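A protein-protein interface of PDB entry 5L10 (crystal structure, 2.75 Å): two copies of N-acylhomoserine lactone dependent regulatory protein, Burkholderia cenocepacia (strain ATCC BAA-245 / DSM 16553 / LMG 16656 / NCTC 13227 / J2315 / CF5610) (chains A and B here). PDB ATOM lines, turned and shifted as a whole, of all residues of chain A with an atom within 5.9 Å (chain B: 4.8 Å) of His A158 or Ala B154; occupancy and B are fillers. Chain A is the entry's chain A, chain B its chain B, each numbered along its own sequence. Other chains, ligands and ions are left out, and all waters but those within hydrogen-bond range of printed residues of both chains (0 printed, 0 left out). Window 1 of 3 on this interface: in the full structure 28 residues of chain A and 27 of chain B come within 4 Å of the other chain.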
ATOM      1  N   PHE A  13      29.577 -34.994  15.641  1.00  0.00           N
ATOM      2  CA  PHE A  13      29.813 -33.661  16.180  1.00  0.00           C
ATOM      3  C   PHE A  13      30.623 -33.698  17.468  1.00  0.00           C
ATOM      4  O   PHE A  13      31.388 -32.767  17.740  1.00  0.00           O
ATOM      5  CB  PHE A  13      28.484 -32.939  16.390  1.00  0.00           C
ATOM      6  CG  PHE A  13      27.975 -32.273  15.150  1.00  0.00           C
ATOM      7  CD1 PHE A  13      28.204 -30.924  14.927  1.00  0.00           C
ATOM      8  CD2 PHE A  13      27.308 -33.003  14.183  1.00  0.00           C
ATOM      9  CE1 PHE A  13      27.751 -30.312  13.772  1.00  0.00           C
ATOM     10  CE2 PHE A  13      26.856 -32.397  13.031  1.00  0.00           C
ATOM     11  CZ  PHE A  13      27.075 -31.051  12.825  1.00  0.00           C
ATOM     12  N   CYS A 153      22.103 -34.499   5.854  1.00  0.00           N
ATOM     13  CA  CYS A 153      23.121 -33.956   4.961  1.00  0.00           C
ATOM     14  C   CYS A 153      23.396 -32.492   5.266  1.00  0.00           C
ATOM     15  O   CYS A 153      24.548 -32.044   5.201  1.00  0.00           O
ATOM     16  CB  CYS A 153      22.691 -34.131   3.508  1.00  0.00           C
ATOM     17  SG  CYS A 153      22.867 -35.811   2.914  1.00  0.00           S
ATOM     18  N   ALA A 154      22.347 -31.729   5.586  1.00  0.00           N
ATOM     19  CA  ALA A 154      22.522 -30.349   6.025  1.00  0.00           C
ATOM     20  C   ALA A 154      23.433 -30.281   7.242  1.00  0.00           C
ATOM     21  O   ALA A 154      24.339 -29.443   7.315  1.00  0.00           O
ATOM     22  CB  ALA A 154      21.161 -29.734   6.343  1.00  0.00           C
ATOM     23  N   SER A 155      23.196 -31.163   8.211  1.00  0.00           N
ATOM     24  CA  SER A 155      24.047 -31.236   9.391  1.00  0.00           C
ATOM     25  C   SER A 155      25.509 -31.438   9.000  1.00  0.00           C
ATOM     26  O   SER A 155      26.387 -30.678   9.423  1.00  0.00           O
ATOM     27  CB  SER A 155      23.554 -32.361  10.300  1.00  0.00           C
ATOM     28  OG  SER A 155      24.319 -32.439  11.481  1.00  0.00           O
ATOM     29  N   LEU A 156      25.784 -32.450   8.171  1.00  0.00           N
ATOM     30  CA  LEU A 156      27.156 -32.715   7.739  1.00  0.00           C
ATOM     31  C   LEU A 156      27.738 -31.538   6.971  1.00  0.00           C
ATOM     32  O   LEU A 156      28.938 -31.251   7.067  1.00  0.00           O
ATOM     33  CB  LEU A 156      27.204 -33.968   6.867  1.00  0.00           C
ATOM     34  CG  LEU A 156      27.225 -35.307   7.589  1.00  0.00           C
ATOM     35  CD1 LEU A 156      27.386 -36.439   6.582  1.00  0.00           C
ATOM     36  CD2 LEU A 156      28.359 -35.301   8.591  1.00  0.00           C
ATOM     37  N   SER A 157      26.904 -30.861   6.183  1.00  0.00           N
ATOM     38  CA  SER A 157      27.374 -29.737   5.385  1.00  0.00           C
ATOM     39  C   SER A 157      27.808 -28.579   6.274  1.00  0.00           C
ATOM     40  O   SER A 157      28.860 -27.968   6.052  1.00  0.00           O
ATOM     41  CB  SER A 157      26.278 -29.302   4.421  1.00  0.00           C
ATOM     42  OG  SER A 157      26.698 -28.182   3.680  1.00  0.00           O
ATOM     43  N   HIS A 158      26.999 -28.255   7.285  1.00  0.00           N
ATOM     44  CA  HIS A 158      27.405 -27.254   8.264  1.00  0.00           C
ATOM     45  C   HIS A 158      28.686 -27.674   8.969  1.00  0.00           C
ATOM     46  O   HIS A 158      29.565 -26.845   9.223  1.00  0.00           O
ATOM     47  CB  HIS A 158      26.281 -27.026   9.278  1.00  0.00           C
ATOM     48  CG  HIS A 158      26.712 -26.289  10.511  1.00  0.00           C
ATOM     49  ND1 HIS A 158      27.389 -26.898  11.546  1.00  0.00           N
ATOM     50  CD2 HIS A 158      26.547 -24.997  10.882  1.00  0.00           C
ATOM     51  CE1 HIS A 158      27.632 -26.013  12.497  1.00  0.00           C
ATOM     52  NE2 HIS A 158      27.131 -24.851  12.118  1.00  0.00           N
ATOM     53  N   ALA A 159      28.809 -28.963   9.285  1.00  0.00           N
ATOM     54  CA  ALA A 159      29.985 -29.445  10.002  1.00  0.00           C
ATOM     55  C   ALA A 159      31.245 -29.301   9.162  1.00  0.00           C
ATOM     56  O   ALA A 159      32.305 -28.931   9.680  1.00  0.00           O
ATOM     57  CB  ALA A 159      29.784 -30.901  10.418  1.00  0.00           C
ATOM     58  N   ALA A 160      31.154 -29.599   7.864  1.00  0.00           N
ATOM     59  CA  ALA A 160      32.325 -29.480   7.003  1.00  0.00           C
ATOM     60  C   ALA A 160      32.766 -28.029   6.884  1.00  0.00           C
ATOM     61  O   ALA A 160      33.963 -27.725   6.953  1.00  0.00           O
ATOM     62  CB  ALA A 160      32.024 -30.068   5.624  1.00  0.00           C
ATOM     63  N   HIS A 161      31.808 -27.119   6.726  1.00  0.00           N
ATOM     64  CA  HIS A 161      32.147 -25.716   6.546  1.00  0.00           C
ATOM     65  C   HIS A 161      32.630 -25.082   7.843  1.00  0.00           C
ATOM     66  O   HIS A 161      33.437 -24.146   7.810  1.00  0.00           O
ATOM     67  CB  HIS A 161      30.939 -24.970   5.988  1.00  0.00           C
ATOM     68  CG  HIS A 161      30.476 -25.492   4.663  1.00  0.00           C
ATOM     69  ND1 HIS A 161      31.348 -25.975   3.711  1.00  0.00           N
ATOM     70  CD2 HIS A 161      29.235 -25.622   4.138  1.00  0.00           C
ATOM     71  CE1 HIS A 161      30.664 -26.371   2.652  1.00  0.00           C
ATOM     72  NE2 HIS A 161      29.380 -26.170   2.886  1.00  0.00           N
ATOM     73  N   ALA A 162      32.167 -25.583   8.988  1.00  0.00           N
ATOM     74  CA  ALA A 162      32.517 -24.982  10.268  1.00  0.00           C
ATOM     75  C   ALA A 162      33.746 -25.612  10.908  1.00  0.00           C
ATOM     76  O   ALA A 162      34.475 -24.924  11.632  1.00  0.00           O
ATOM     77  CB  ALA A 162      31.337 -25.074  11.238  1.00  0.00           C
ATOM     78  N   TYR A 163      33.999 -26.897  10.659  1.00  0.00           N
ATOM     79  CA  TYR A 163      35.079 -27.602  11.334  1.00  0.00           C
ATOM     80  C   TYR A 163      36.211 -28.042  10.417  1.00  0.00           C
ATOM     81  O   TYR A 163      37.330 -28.230  10.904  1.00  0.00           O
ATOM     82  CB  TYR A 163      34.534 -28.837  12.066  1.00  0.00           C
ATOM     83  CG  TYR A 163      33.573 -28.508  13.184  1.00  0.00           C
ATOM     84  CD1 TYR A 163      34.032 -28.302  14.479  1.00  0.00           C
ATOM     85  CD2 TYR A 163      32.210 -28.404  12.946  1.00  0.00           C
ATOM     86  CE1 TYR A 163      33.156 -28.004  15.508  1.00  0.00           C
ATOM     87  CE2 TYR A 163      31.328 -28.106  13.968  1.00  0.00           C
ATOM     88  CZ  TYR A 163      31.806 -27.908  15.246  1.00  0.00           C
ATOM     89  OH  TYR A 163      30.931 -27.609  16.264  1.00  0.00           O
ATOM     90  N   PRO B  91      29.624 -22.338  15.818  1.00  0.00           N
ATOM     91  CA  PRO B  91      28.551 -21.673  16.570  1.00  0.00           C
ATOM     92  C   PRO B  91      29.047 -21.063  17.875  1.00  0.00           C
ATOM     93  O   PRO B  91      30.080 -21.448  18.428  1.00  0.00           O
ATOM     94  CB  PRO B  91      27.550 -22.804  16.840  1.00  0.00           C
ATOM     95  CG  PRO B  91      27.847 -23.834  15.796  1.00  0.00           C
ATOM     96  CD  PRO B  91      29.323 -23.758  15.566  1.00  0.00           C
ATOM     97  N   HIS B 120      24.845 -18.652  15.083  1.00  0.00           N
ATOM     98  CA  HIS B 120      25.773 -19.119  14.068  1.00  0.00           C
ATOM     99  C   HIS B 120      25.655 -18.229  12.841  1.00  0.00           C
ATOM    100  O   HIS B 120      24.547 -17.888  12.417  1.00  0.00           O
ATOM    101  CB  HIS B 120      25.511 -20.577  13.689  1.00  0.00           C
ATOM    102  CG  HIS B 120      26.364 -21.058  12.561  1.00  0.00           C
ATOM    103  ND1 HIS B 120      27.681 -21.428  12.727  1.00  0.00           N
ATOM    104  CD2 HIS B 120      26.095 -21.206  11.242  1.00  0.00           C
ATOM    105  CE1 HIS B 120      28.183 -21.796  11.562  1.00  0.00           C
ATOM    106  NE2 HIS B 120      27.241 -21.669  10.645  1.00  0.00           N
ATOM    107  N   LEU B 149      22.240 -31.039  21.026  1.00  0.00           N
ATOM    108  CA  LEU B 149      21.639 -29.984  20.219  1.00  0.00           C
ATOM    109  C   LEU B 149      22.479 -29.601  19.010  1.00  0.00           C
ATOM    110  O   LEU B 149      21.979 -28.879  18.143  1.00  0.00           O
ATOM    111  CB  LEU B 149      21.398 -28.726  21.062  1.00  0.00           C
ATOM    112  CG  LEU B 149      20.180 -28.625  21.985  1.00  0.00           C
ATOM    113  CD1 LEU B 149      20.245 -27.331  22.795  1.00  0.00           C
ATOM    114  CD2 LEU B 149      18.884 -28.700  21.196  1.00  0.00           C
ATOM    115  N   ARG B 150      23.732 -30.058  18.930  1.00  0.00           N
ATOM    116  CA  ARG B 150      24.625 -29.610  17.866  1.00  0.00           C
ATOM    117  C   ARG B 150      24.107 -30.018  16.495  1.00  0.00           C
ATOM    118  O   ARG B 150      23.893 -29.171  15.620  1.00  0.00           O
ATOM    119  CB  ARG B 150      26.032 -30.162  18.085  1.00  0.00           C
ATOM    120  CG  ARG B 150      26.801 -29.467  19.181  1.00  0.00           C
ATOM    121  CD  ARG B 150      28.294 -29.636  18.989  1.00  0.00           C
ATOM    122  NE  ARG B 150      29.034 -29.032  20.088  1.00  0.00           N
ATOM    123  CZ  ARG B 150      29.350 -29.672  21.209  1.00  0.00           C
ATOM    124  NH1 ARG B 150      28.992 -30.939  21.371  1.00  0.00           N
ATOM    125  NH2 ARG B 150      30.026 -29.048  22.164  1.00  0.00           N
ATOM    126  N   ALA B 151      23.918 -31.320  16.282  1.00  0.00           N
ATOM    127  CA  ALA B 151      23.458 -31.786  14.977  1.00  0.00           C
ATOM    128  C   ALA B 151      22.126 -31.166  14.568  1.00  0.00           C
ATOM    129  O   ALA B 151      22.021 -30.696  13.421  1.00  0.00           O
ATOM    130  CB  ALA B 151      23.408 -33.316  14.961  1.00  0.00           C
ATOM    131  N   PRO B 152      21.095 -31.102  15.421  1.00  0.00           N
ATOM    132  CA  PRO B 152      19.859 -30.432  14.982  1.00  0.00           C
ATOM    133  C   PRO B 152      20.043 -28.950  14.704  1.00  0.00           C
ATOM    134  O   PRO B 152      19.475 -28.440  13.731  1.00  0.00           O
ATOM    135  CB  PRO B 152      18.890 -30.676  16.148  1.00  0.00           C
ATOM    136  CG  PRO B 152      19.445 -31.839  16.872  1.00  0.00           C
ATOM    137  CD  PRO B 152      20.926 -31.717  16.750  1.00  0.00           C
ATOM    138  N   CYS B 153      20.819 -28.239  15.531  1.00  0.00           N
ATOM    139  CA  CYS B 153      21.012 -26.809  15.300  1.00  0.00           C
ATOM    140  C   CYS B 153      21.866 -26.549  14.067  1.00  0.00           C
ATOM    141  O   CYS B 153      21.682 -25.529  13.393  1.00  0.00           O
ATOM    142  CB  CYS B 153      21.640 -26.150  16.525  1.00  0.00           C
ATOM    143  SG  CYS B 153      20.521 -25.975  17.928  1.00  0.00           S
ATOM    144  N   ALA B 154      22.805 -27.447  13.765  1.00  0.00           N
ATOM    145  CA  ALA B 154      23.546 -27.346  12.514  1.00  0.00           C
ATOM    146  C   ALA B 154      22.605 -27.402  11.317  1.00  0.00           C
ATOM    147  O   ALA B 154      22.737 -26.611  10.376  1.00  0.00           O
ATOM    148  CB  ALA B 154      24.591 -28.458  12.433  1.00  0.00           C
ATOM    149  N   SER B 155      21.640 -28.327  11.338  1.00  0.00           N
ATOM    150  CA  SER B 155      20.657 -28.391  10.262  1.00  0.00           C
ATOM    151  C   SER B 155      19.866 -27.098  10.162  1.00  0.00           C
ATOM    152  O   SER B 155      19.588 -26.615   9.058  1.00  0.00           O
ATOM    153  CB  SER B 155      19.712 -29.571  10.475  1.00  0.00           C
ATOM    154  OG  SER B 155      20.421 -30.793  10.464  1.00  0.00           O
ATOM    155  N   LEU B 156      19.486 -26.523  11.307  1.00  0.00           N
ATOM    156  CA  LEU B 156      18.746 -25.267  11.291  1.00  0.00           C
ATOM    157  C   LEU B 156      19.590 -24.138  10.718  1.00  0.00           C
ATOM    158  O   LEU B 156      19.085 -23.304   9.960  1.00  0.00           O
ATOM    159  CB  LEU B 156      18.271 -24.915  12.695  1.00  0.00           C
ATOM    160  CG  LEU B 156      16.971 -25.590  13.118  1.00  0.00           C
ATOM    161  CD1 LEU B 156      16.434 -24.965  14.398  1.00  0.00           C
ATOM    162  CD2 LEU B 156      15.953 -25.490  11.997  1.00  0.00           C
ATOM    163  N   SER B 157      20.876 -24.095  11.073  1.00  0.00           N
ATOM    164  CA  SER B 157      21.778 -23.109  10.487  1.00  0.00           C
ATOM    165  C   SER B 157      21.830 -23.250   8.975  1.00  0.00           C
ATOM    166  O   SER B 157      21.614 -22.277   8.242  1.00  0.00           O
ATOM    167  CB  SER B 157      23.177 -23.253  11.084  1.00  0.00           C
ATOM    168  OG  SER B 157      23.213 -22.755  12.408  1.00  0.00           O
ATOM    169  N   HIS B 158      22.121 -24.459   8.488  1.00  0.00           N
ATOM    170  CA  HIS B 158      22.103 -24.698   7.050  1.00  0.00           C
ATOM    171  C   HIS B 158      20.766 -24.293   6.447  1.00  0.00           C
ATOM    172  O   HIS B 158      20.722 -23.632   5.403  1.00  0.00           O
ATOM    173  CB  HIS B 158      22.396 -26.168   6.750  1.00  0.00           C
ATOM    174  CG  HIS B 158      22.188 -26.543   5.315  1.00  0.00           C
ATOM    175  ND1 HIS B 158      23.201 -26.501   4.380  1.00  0.00           N
ATOM    176  CD2 HIS B 158      21.081 -26.955   4.652  1.00  0.00           C
ATOM    177  CE1 HIS B 158      22.727 -26.882   3.207  1.00  0.00           C
ATOM    178  NE2 HIS B 158      21.444 -27.164   3.345  1.00  0.00           N
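Of the 12 printed residues of chain B, 8 touch a printed residue of chain A. Printed residues of chain B that touch a printed residue of chain A: Pro B91, His B120, Arg B150, Ala B151, Ala B154, Ser B155, Ser B157 and His B158. Printed residues of chain A that touch a printed residue of chain B: Phe A13, Ala A154, Ser A155, Ser A157 and His A158. Among the printed residues, 11 pairs touch across the chains.
OG of Ser A155 lies within hydrogen-bond range of O of Ala B151 (3.5 Å).
Of the printed residues of chain B, Ala A154 touches His B158. Of the printed residues of chain A, Ala B151 touches Phe A13 (3.96 Å) and Ser A155 (3.5 Å). Of chain A, only Phe A13 and His A158 come within 4 Å of Ala B154. The nearest residue of chain B that does not touch His A158 is His B158 (4.7 Å). The nearest printed residue of chain B that does not touch Phe A13 is Ser B155 (6.3 Å).
OG of Ser A157 lies within hydrogen-bond range of NE2 of His A161 (3.4 Å). OG of Ser B155 sits at hydrogen-bond distance from O of Ala B151. O of Cys B153 sits at hydrogen-bond distance from OG of Ser B157, at 3.3 Å.
Among the printed residues, pairs that only touch across the chains: Ala A154 with His B158, His A158 with His B120, His A158 with Ala B154, Ser A155 with Ser B155, Phe A13 with Ala B154, His A158 with Ser B157, His A158 with Pro B91, Phe A13 with Arg B150, Ser A157 with His B158 and Phe A13 with Ala B151.
Ala A154 touches His B158, and with the chains exchanged His A158 touches Ala B154. Ser B155 touches its own counterpart, Ser A155. Ser A157 touches His B158, and with the chains exchanged His A158 touches Ser B157. 6 positions are printed for both chains.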
